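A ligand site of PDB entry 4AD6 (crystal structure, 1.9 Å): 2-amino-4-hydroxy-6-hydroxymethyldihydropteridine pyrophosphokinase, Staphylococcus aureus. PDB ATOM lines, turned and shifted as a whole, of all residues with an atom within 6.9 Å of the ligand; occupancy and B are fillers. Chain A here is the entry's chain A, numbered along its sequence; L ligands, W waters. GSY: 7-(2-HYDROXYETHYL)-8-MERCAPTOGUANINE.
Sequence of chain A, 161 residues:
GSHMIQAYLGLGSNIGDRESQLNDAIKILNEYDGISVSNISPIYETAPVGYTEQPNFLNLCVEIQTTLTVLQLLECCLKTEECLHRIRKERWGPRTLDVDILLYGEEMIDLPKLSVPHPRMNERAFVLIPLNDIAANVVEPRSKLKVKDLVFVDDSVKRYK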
ATOM      1  N   GLY A  10      -8.906 -21.358  22.244  1.00  0.00           N
ATOM      2  CA  GLY A  10      -8.759 -20.309  23.250  1.00  0.00           C
ATOM      3  C   GLY A  10     -10.074 -19.573  23.300  1.00  0.00           C
ATOM      4  O   GLY A  10     -10.544 -19.100  22.280  1.00  0.00           O
ATOM      5  N   LEU A  11     -10.652 -19.461  24.498  1.00  0.00           N
ATOM      6  CA  LEU A  11     -11.886 -18.780  24.709  1.00  0.00           C
ATOM      7  C   LEU A  11     -11.740 -17.624  25.690  1.00  0.00           C
ATOM      8  O   LEU A  11     -10.932 -17.697  26.646  1.00  0.00           O
ATOM      9  CB  LEU A  11     -12.959 -19.724  25.205  1.00  0.00           C
ATOM     10  CG  LEU A  11     -13.487 -20.775  24.206  1.00  0.00           C
ATOM     11  CD1 LEU A  11     -12.546 -21.932  23.991  1.00  0.00           C
ATOM     12  CD2 LEU A  11     -14.798 -21.281  24.702  1.00  0.00           C
ATOM     13  N   GLY A  12     -12.533 -16.589  25.450  1.00  0.00           N
ATOM     14  CA  GLY A  12     -12.450 -15.331  26.248  1.00  0.00           C
ATOM     15  C   GLY A  12     -13.754 -14.582  26.305  1.00  0.00           C
ATOM     16  O   GLY A  12     -14.436 -14.529  25.304  1.00  0.00           O
ATOM     17  N   SER A  13     -14.022 -13.897  27.444  1.00  0.00           N
ATOM     18  CA  SER A  13     -15.152 -13.032  27.554  1.00  0.00           C
ATOM     19  C   SER A  13     -14.834 -11.980  28.567  1.00  0.00           C
ATOM     20  O   SER A  13     -14.380 -12.327  29.642  1.00  0.00           O
ATOM     21  CB  SER A  13     -16.357 -13.822  28.014  1.00  0.00           C
ATOM     22  OG  SER A  13     -17.461 -12.949  28.204  1.00  0.00           O
ATOM     23  N   ASN A  14     -15.080 -10.702  28.244  1.00  0.00           N
ATOM     24  CA  ASN A  14     -14.805  -9.639  29.216  1.00  0.00           C
ATOM     25  C   ASN A  14     -15.989  -8.784  29.693  1.00  0.00           C
ATOM     26  O   ASN A  14     -15.806  -7.877  30.522  1.00  0.00           O
ATOM     27  CB  ASN A  14     -13.628  -8.754  28.767  1.00  0.00           C
ATOM     28  CG  ASN A  14     -13.981  -7.789  27.659  1.00  0.00           C
ATOM     29  OD1 ASN A  14     -14.881  -8.021  26.850  1.00  0.00           O
ATOM     30  ND2 ASN A  14     -13.285  -6.684  27.616  1.00  0.00           N
ATOM     31  N   GLU A  45      -8.424 -14.994  35.043  1.00  0.00           N
ATOM     32  CA  GLU A  45      -8.752 -13.611  34.825  1.00  0.00           C
ATOM     33  C   GLU A  45      -7.530 -12.903  34.320  1.00  0.00           C
ATOM     34  O   GLU A  45      -6.497 -12.985  34.913  1.00  0.00           O
ATOM     35  CB  GLU A  45      -9.360 -12.990  36.105  1.00  0.00           C
ATOM     36  CG  GLU A  45      -9.625 -11.526  35.925  1.00  0.00           C
ATOM     37  CD  GLU A  45     -10.508 -10.931  37.005  1.00  0.00           C
ATOM     38  OE1 GLU A  45     -10.006 -10.798  38.162  1.00  0.00           O
ATOM     39  OE2 GLU A  45     -11.680 -10.560  36.706  1.00  0.00           O
ATOM     40  N   THR A  46      -7.637 -12.222  33.166  1.00  0.00           N
ATOM     41  CA  THR A  46      -6.454 -11.603  32.541  1.00  0.00           C
ATOM     42  C   THR A  46      -6.668 -10.119  32.220  1.00  0.00           C
ATOM     43  O   THR A  46      -7.755  -9.695  31.831  1.00  0.00           O
ATOM     44  CB  THR A  46      -6.110 -12.309  31.217  1.00  0.00           C
ATOM     45  OG1 THR A  46      -7.270 -12.314  30.386  1.00  0.00           O
ATOM     46  CG2 THR A  46      -5.618 -13.782  31.485  1.00  0.00           C
ATOM     47  N   ALA A  47      -5.621  -9.328  32.366  1.00  0.00           N
ATOM     48  CA  ALA A  47      -5.728  -7.914  32.002  1.00  0.00           C
ATOM     49  C   ALA A  47      -5.865  -7.792  30.463  1.00  0.00           C
ATOM     50  O   ALA A  47      -5.250  -8.590  29.716  1.00  0.00           O
ATOM     51  CB  ALA A  47      -4.542  -7.091  32.553  1.00  0.00           C
ATOM     52  N   PRO A  48      -6.734  -6.848  30.002  1.00  0.00           N
ATOM     53  CA  PRO A  48      -6.992  -6.670  28.582  1.00  0.00           C
ATOM     54  C   PRO A  48      -5.714  -6.378  27.777  1.00  0.00           C
ATOM     55  O   PRO A  48      -4.908  -5.527  28.195  1.00  0.00           O
ATOM     56  CB  PRO A  48      -7.932  -5.463  28.519  1.00  0.00           C
ATOM     57  CG  PRO A  48      -7.834  -4.809  29.865  1.00  0.00           C
ATOM     58  CD  PRO A  48      -7.521  -5.915  30.854  1.00  0.00           C
ATOM     59  N   VAL A  49      -5.546  -7.092  26.653  1.00  0.00           N
ATOM     60  CA  VAL A  49      -4.436  -6.859  25.729  1.00  0.00           C
ATOM     61  C   VAL A  49      -5.021  -6.172  24.484  1.00  0.00           C
ATOM     62  O   VAL A  49      -6.068  -6.554  24.019  1.00  0.00           O
ATOM     63  CB  VAL A  49      -3.761  -8.204  25.328  1.00  0.00           C
ATOM     64  CG1 VAL A  49      -2.651  -8.014  24.260  1.00  0.00           C
ATOM     65  CG2 VAL A  49      -3.306  -8.970  26.590  1.00  0.00           C
ATOM     66  N   GLY A  50      -4.325  -5.213  23.888  1.00  0.00           N
ATOM     67  CA  GLY A  50      -4.930  -4.417  22.764  1.00  0.00           C
ATOM     68  C   GLY A  50      -5.377  -3.052  23.288  1.00  0.00           C
ATOM     69  O   GLY A  50      -4.577  -2.221  23.618  1.00  0.00           O
ATOM     70  N   TYR A  51      -6.675  -2.838  23.476  1.00  0.00           N
ATOM     71  CA  TYR A  51      -7.098  -1.689  24.222  1.00  0.00           C
ATOM     72  C   TYR A  51      -7.026  -1.938  25.702  1.00  0.00           C
ATOM     73  O   TYR A  51      -7.606  -2.882  26.225  1.00  0.00           O
ATOM     74  CB  TYR A  51      -8.538  -1.374  23.955  1.00  0.00           C
ATOM     75  CG  TYR A  51      -8.868  -1.151  22.510  1.00  0.00           C
ATOM     76  CD1 TYR A  51      -8.020  -0.459  21.676  1.00  0.00           C
ATOM     77  CD2 TYR A  51     -10.070  -1.647  21.999  1.00  0.00           C
ATOM     78  CE1 TYR A  51      -8.343  -0.272  20.341  1.00  0.00           C
ATOM     79  CE2 TYR A  51     -10.421  -1.444  20.693  1.00  0.00           C
ATOM     80  CZ  TYR A  51      -9.571  -0.748  19.878  1.00  0.00           C
ATOM     81  OH  TYR A  51      -9.952  -0.585  18.573  1.00  0.00           O
ATOM     82  N   GLN A  54     -10.698  -1.394  28.904  1.00  0.00           N
ATOM     83  CA  GLN A  54     -11.835  -2.315  28.782  1.00  0.00           C
ATOM     84  C   GLN A  54     -11.749  -3.353  29.947  1.00  0.00           C
ATOM     85  O   GLN A  54     -10.713  -3.464  30.587  1.00  0.00           O
ATOM     86  CB  GLN A  54     -11.825  -3.015  27.409  1.00  0.00           C
ATOM     87  CG  GLN A  54     -10.650  -3.976  27.235  1.00  0.00           C
ATOM     88  CD  GLN A  54     -10.627  -4.628  25.891  1.00  0.00           C
ATOM     89  OE1 GLN A  54     -11.657  -5.009  25.383  1.00  0.00           O
ATOM     90  NE2 GLN A  54      -9.478  -4.674  25.274  1.00  0.00           N
ATOM     91  N   PRO A  55     -12.846  -4.086  30.243  1.00  0.00           N
ATOM     92  CA  PRO A  55     -12.799  -4.959  31.414  1.00  0.00           C
ATOM     93  C   PRO A  55     -11.851  -6.123  31.302  1.00  0.00           C
ATOM     94  O   PRO A  55     -11.521  -6.587  30.191  1.00  0.00           O
ATOM     95  CB  PRO A  55     -14.267  -5.487  31.546  1.00  0.00           C
ATOM     96  CG  PRO A  55     -15.109  -4.396  30.876  1.00  0.00           C
ATOM     97  CD  PRO A  55     -14.233  -3.866  29.737  1.00  0.00           C
ATOM     98  N   ASN A  56     -11.494  -6.661  32.447  1.00  0.00           N
ATOM     99  CA  ASN A  56     -10.700  -7.855  32.435  1.00  0.00           C
ATOM    100  C   ASN A  56     -11.405  -8.997  31.768  1.00  0.00           C
ATOM    101  O   ASN A  56     -12.657  -9.227  31.940  1.00  0.00           O
ATOM    102  CB  ASN A  56     -10.332  -8.287  33.864  1.00  0.00           C
ATOM    103  CG  ASN A  56      -9.835  -7.140  34.699  1.00  0.00           C
ATOM    104  OD1 ASN A  56      -9.012  -6.357  34.226  1.00  0.00           O
ATOM    105  ND2 ASN A  56     -10.288  -7.084  35.962  1.00  0.00           N
ATOM    106  N   PHE A  57     -10.614  -9.806  31.104  1.00  0.00           N
ATOM    107  CA  PHE A  57     -11.194 -11.023  30.506  1.00  0.00           C
ATOM    108  C   PHE A  57     -11.143 -12.207  31.480  1.00  0.00           C
ATOM    109  O   PHE A  57     -10.281 -12.240  32.341  1.00  0.00           O
ATOM    110  CB  PHE A  57     -10.412 -11.482  29.260  1.00  0.00           C
ATOM    111  CG  PHE A  57     -10.631 -10.639  28.056  1.00  0.00           C
ATOM    112  CD1 PHE A  57     -10.051  -9.357  27.940  1.00  0.00           C
ATOM    113  CD2 PHE A  57     -11.437 -11.103  27.037  1.00  0.00           C
ATOM    114  CE1 PHE A  57     -10.287  -8.573  26.792  1.00  0.00           C
ATOM    115  CE2 PHE A  57     -11.703 -10.317  25.901  1.00  0.00           C
ATOM    116  CZ  PHE A  57     -11.121  -9.062  25.801  1.00  0.00           C
ATOM    117  N   LEU A  58     -12.083 -13.147  31.308  1.00  0.00           N
ATOM    118  CA  LEU A  58     -11.873 -14.543  31.703  1.00  0.00           C
ATOM    119  C   LEU A  58     -11.464 -15.265  30.439  1.00  0.00           C
ATOM    120  O   LEU A  58     -12.058 -15.068  29.388  1.00  0.00           O
ATOM    121  CB  LEU A  58     -13.155 -15.159  32.345  1.00  0.00           C
ATOM    122  CG  LEU A  58     -13.651 -14.449  33.648  1.00  0.00           C
ATOM    123  CD1 LEU A  58     -14.792 -15.234  34.308  1.00  0.00           C
ATOM    124  CD2 LEU A  58     -12.576 -14.227  34.672  1.00  0.00           C
ATOM    125  N   ASN A  59     -10.379 -16.042  30.538  1.00  0.00           N
ATOM    126  CA  ASN A  59      -9.829 -16.867  29.452  1.00  0.00           C
ATOM    127  C   ASN A  59      -9.684 -18.317  29.925  1.00  0.00           C
ATOM    128  O   ASN A  59      -9.374 -18.595  31.086  1.00  0.00           O
ATOM    129  CB  ASN A  59      -8.428 -16.311  29.083  1.00  0.00           C
ATOM    130  CG  ASN A  59      -8.496 -15.096  28.154  1.00  0.00           C
ATOM    131  OD1 ASN A  59      -8.093 -13.975  28.519  1.00  0.00           O
ATOM    132  ND2 ASN A  59      -9.021 -15.287  26.971  1.00  0.00           N
ATOM    133  N   ASP A  98     -14.973 -14.522  22.637  1.00  0.00           N
ATOM    134  CA  ASP A  98     -14.007 -14.835  21.570  1.00  0.00           C
ATOM    135  C   ASP A  98     -13.660 -16.324  21.637  1.00  0.00           C
ATOM    136  O   ASP A  98     -13.518 -16.888  22.720  1.00  0.00           O
ATOM    137  CB  ASP A  98     -12.748 -13.987  21.730  1.00  0.00           C
ATOM    138  CG  ASP A  98     -13.079 -12.502  21.736  1.00  0.00           C
ATOM    139  OD1 ASP A  98     -13.424 -11.985  20.636  1.00  0.00           O
ATOM    140  OD2 ASP A  98     -13.068 -11.930  22.859  1.00  0.00           O
ATOM    141  N   VAL A  99     -13.605 -16.966  20.473  1.00  0.00           N
ATOM    142  CA  VAL A  99     -13.181 -18.393  20.355  1.00  0.00           C
ATOM    143  C   VAL A  99     -12.253 -18.482  19.148  1.00  0.00           C
ATOM    144  O   VAL A  99     -12.651 -18.117  18.014  1.00  0.00           O
ATOM    145  CB  VAL A  99     -14.326 -19.342  19.973  1.00  0.00           C
ATOM    146  CG1 VAL A  99     -13.831 -20.814  20.149  1.00  0.00           C
ATOM    147  CG2 VAL A  99     -15.595 -18.992  20.714  1.00  0.00           C
ATOM    148  N   ASP A 100     -10.995 -18.854  19.399  1.00  0.00           N
ATOM    149  CA  ASP A 100      -9.909 -18.846  18.436  1.00  0.00           C
ATOM    150  C   ASP A 100      -9.402 -20.294  18.358  1.00  0.00           C
ATOM    151  O   ASP A 100      -9.374 -20.993  19.389  1.00  0.00           O
ATOM    152  CB  ASP A 100      -8.722 -18.049  19.003  1.00  0.00           C
ATOM    153  CG  ASP A 100      -8.786 -16.596  18.678  1.00  0.00           C
ATOM    154  OD1 ASP A 100      -9.047 -16.260  17.500  1.00  0.00           O
ATOM    155  OD2 ASP A 100      -8.537 -15.761  19.592  1.00  0.00           O
ATOM    156  N   ARG A 124       0.987 -14.149  23.902  1.00  0.00           N
ATOM    157  CA  ARG A 124      -0.242 -14.009  24.667  1.00  0.00           C
ATOM    158  C   ARG A 124      -0.253 -14.965  25.882  1.00  0.00           C
ATOM    159  O   ARG A 124      -0.539 -16.192  25.770  1.00  0.00           O
ATOM    160  CB  ARG A 124      -1.461 -14.178  23.744  1.00  0.00           C
ATOM    161  CG  ARG A 124      -1.613 -12.926  22.895  1.00  0.00           C
ATOM    162  CD  ARG A 124      -1.996 -13.102  21.452  1.00  0.00           C
ATOM    163  NE  ARG A 124      -1.621 -11.827  20.817  1.00  0.00           N
ATOM    164  CZ  ARG A 124      -1.878 -11.468  19.562  1.00  0.00           C
ATOM    165  NH1 ARG A 124      -2.522 -12.289  18.725  1.00  0.00           N
ATOM    166  NH2 ARG A 124      -1.470 -10.280  19.129  1.00  0.00           N
ATOM    167  N   PHE A 126      -2.408 -14.839  28.165  1.00  0.00           N
ATOM    168  CA  PHE A 126      -3.826 -15.224  28.426  1.00  0.00           C
ATOM    169  C   PHE A 126      -4.199 -16.483  27.638  1.00  0.00           C
ATOM    170  O   PHE A 126      -5.202 -17.133  27.980  1.00  0.00           O
ATOM    171  CB  PHE A 126      -4.739 -14.060  28.175  1.00  0.00           C
ATOM    172  CG  PHE A 126      -4.940 -13.689  26.697  1.00  0.00           C
ATOM    173  CD1 PHE A 126      -5.821 -14.395  25.923  1.00  0.00           C
ATOM    174  CD2 PHE A 126      -4.340 -12.524  26.154  1.00  0.00           C
ATOM    175  CE1 PHE A 126      -6.063 -14.036  24.574  1.00  0.00           C
ATOM    176  CE2 PHE A 126      -4.630 -12.126  24.841  1.00  0.00           C
ATOM    177  CZ  PHE A 126      -5.470 -12.894  24.068  1.00  0.00           C
ATOM    178  N   VAL A 127      -3.401 -16.779  26.610  1.00  0.00           N
ATOM    179  CA  VAL A 127      -3.488 -18.029  25.893  1.00  0.00           C
ATOM    180  C   VAL A 127      -2.589 -19.059  26.514  1.00  0.00           C
ATOM    181  O   VAL A 127      -3.027 -20.117  26.930  1.00  0.00           O
ATOM    182  CB  VAL A 127      -3.099 -17.886  24.424  1.00  0.00           C
ATOM    183  CG1 VAL A 127      -3.134 -19.290  23.748  1.00  0.00           C
ATOM    184  CG2 VAL A 127      -3.992 -16.857  23.751  1.00  0.00           C
ATOM    185  N   SER A 156      -0.160 -10.221  34.975  1.00  0.00           N
ATOM    186  CA  SER A 156      -1.480  -9.754  34.562  1.00  0.00           C
ATOM    187  C   SER A 156      -2.454 -10.918  34.351  1.00  0.00           C
ATOM    188  O   SER A 156      -3.608 -10.667  34.017  1.00  0.00           O
ATOM    189  CB  SER A 156      -1.383  -8.870  33.296  1.00  0.00           C
ATOM    190  OG  SER A 156      -1.281  -9.594  32.086  1.00  0.00           O
ATOM    191  N   VAL A 157      -2.007 -12.165  34.530  1.00  0.00           N
ATOM    192  CA  VAL A 157      -2.861 -13.348  34.325  1.00  0.00           C
ATOM    193  C   VAL A 157      -2.894 -14.129  35.635  1.00  0.00           C
ATOM    194  O   VAL A 157      -1.841 -14.545  36.107  1.00  0.00           O
ATOM    195  CB  VAL A 157      -2.272 -14.310  33.216  1.00  0.00           C
ATOM    196  CG1 VAL A 157      -2.991 -15.649  33.088  1.00  0.00           C
ATOM    197  CG2 VAL A 157      -2.093 -13.612  31.853  1.00  0.00           C
HETATM  198  O15 GSY L   1      -8.451 -12.321  21.108  1.00  0.00           O
HETATM  199  C14 GSY L   1      -8.985 -12.634  22.378  1.00  0.00           C
HETATM  200  C13 GSY L   1      -9.818 -11.442  22.835  1.00  0.00           C
HETATM  201  N7  GSY L   1      -8.860 -10.531  23.557  1.00  0.00           N
HETATM  202  C5  GSY L   1      -8.347 -10.850  24.755  1.00  0.00           C
HETATM  203  C6  GSY L   1      -8.464 -11.969  25.613  1.00  0.00           C
HETATM  204  O11 GSY L   1      -9.198 -12.951  25.384  1.00  0.00           O
HETATM  205  N1  GSY L   1      -7.788 -11.936  26.822  1.00  0.00           N
HETATM  206  C2  GSY L   1      -6.981 -10.800  27.092  1.00  0.00           C
HETATM  207  N2  GSY L   1      -6.350 -10.672  28.221  1.00  0.00           N
HETATM  208  N3  GSY L   1      -6.903  -9.778  26.259  1.00  0.00           N
HETATM  209  C4  GSY L   1      -7.565  -9.769  25.101  1.00  0.00           C
HETATM  210  N9  GSY L   1      -7.648  -8.854  24.119  1.00  0.00           N
HETATM  211  C8  GSY L   1      -8.437  -9.325  23.202  1.00  0.00           C
HETATM  212  S10 GSY L   1      -8.787  -8.397  21.701  1.00  0.00           S
HETATM  213  O   HOH W   1      -8.440  -5.317  22.386  1.00  0.00           O
HETATM  214  O   HOH W   2      -9.938 -15.376  24.034  1.00  0.00           O
HETATM  215  O   HOH W   3      -6.173 -13.735  20.834  1.00  0.00           O
HETATM  216  O   HOH W   4      -9.439 -13.462  18.826  1.00  0.00           O
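O of Ala 47 is in hydrogen-bond range of N2 of the ligand, 2.8 Å away. OG1 of Thr 46 is in hydrogen-bond range of N2 of the ligand (2.9 Å). N1 of the ligand sits at hydrogen-bond distance from OD1 of Asn 59. The backbone NH (N) of Val 49 is in hydrogen-bond range of a nitrogen (N3) of the ligand, 3.0 Å away.
O of Leu 11 sits at hydrogen-bond distance from ND2 of Asn 59 (3.1 Å). The backbone NH (N) of Gly 10 sits at hydrogen-bond distance from the backbone carbonyl oxygen (O) of Asp 100. The backbone NH (N) of Ala 47 sits at hydrogen-bond distance from the backbone carbonyl oxygen (O) of Ser 156. OD1 of Asn 59 is in hydrogen-bond range of OG1 of Thr 46 (2.6 Å). The backbone carbonyl oxygen (O) of Phe 57 lies within hydrogen-bond range of the backbone NH (N) of Thr 46 (2.8 Å). The backbone NH of Asp 98 is in hydrogen-bond range of the backbone carbonyl oxygen of Gly 12, 2.7 Å away.
Water W3 lies within hydrogen-bond range of an oxygen (O15) of the ligand and the side-chain carboxylate of Asp 100. Water W4 bridges the side-chain carboxylate (OD2) of Asp 100 (2.6 Å) and an oxygen (O15) of the ligand (2.7 Å). Water W2 lies within hydrogen-bond range of an oxygen (O11) of the ligand (2.9 Å), the side-chain amide nitrogen of Asn 59 (3.1 Å) and the backbone NH of Gly 12 (3.2 Å). Water W1 lies within hydrogen-bond range of O of Val 49 (3.1 Å), NE2 of Gln 54 (3.1 Å), S10 of the ligand (3.2 Å) and N of Tyr 51 (3.2 Å).
Residues that only touch the ligand: Phe 126 (3.3 Å), Asp 98 (3.3 Å), Phe 57 (3.3 Å), Asp 100 (3.8 Å) and Pro 48 (3.9 Å). Hydrophobic or aromatic side chains within 4 Å of the ligand: Val 49, Phe 57 and Phe 126. Nine residues have an atom within 4 Å of the ligand: Thr 46, Ala 47, Pro 48, Val 49, Phe 57, Asn 59, Asp 98, Asp 100 and Phe 126. The nearest printed residue that does not touch the ligand is Gly 12 (4.1 Å).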
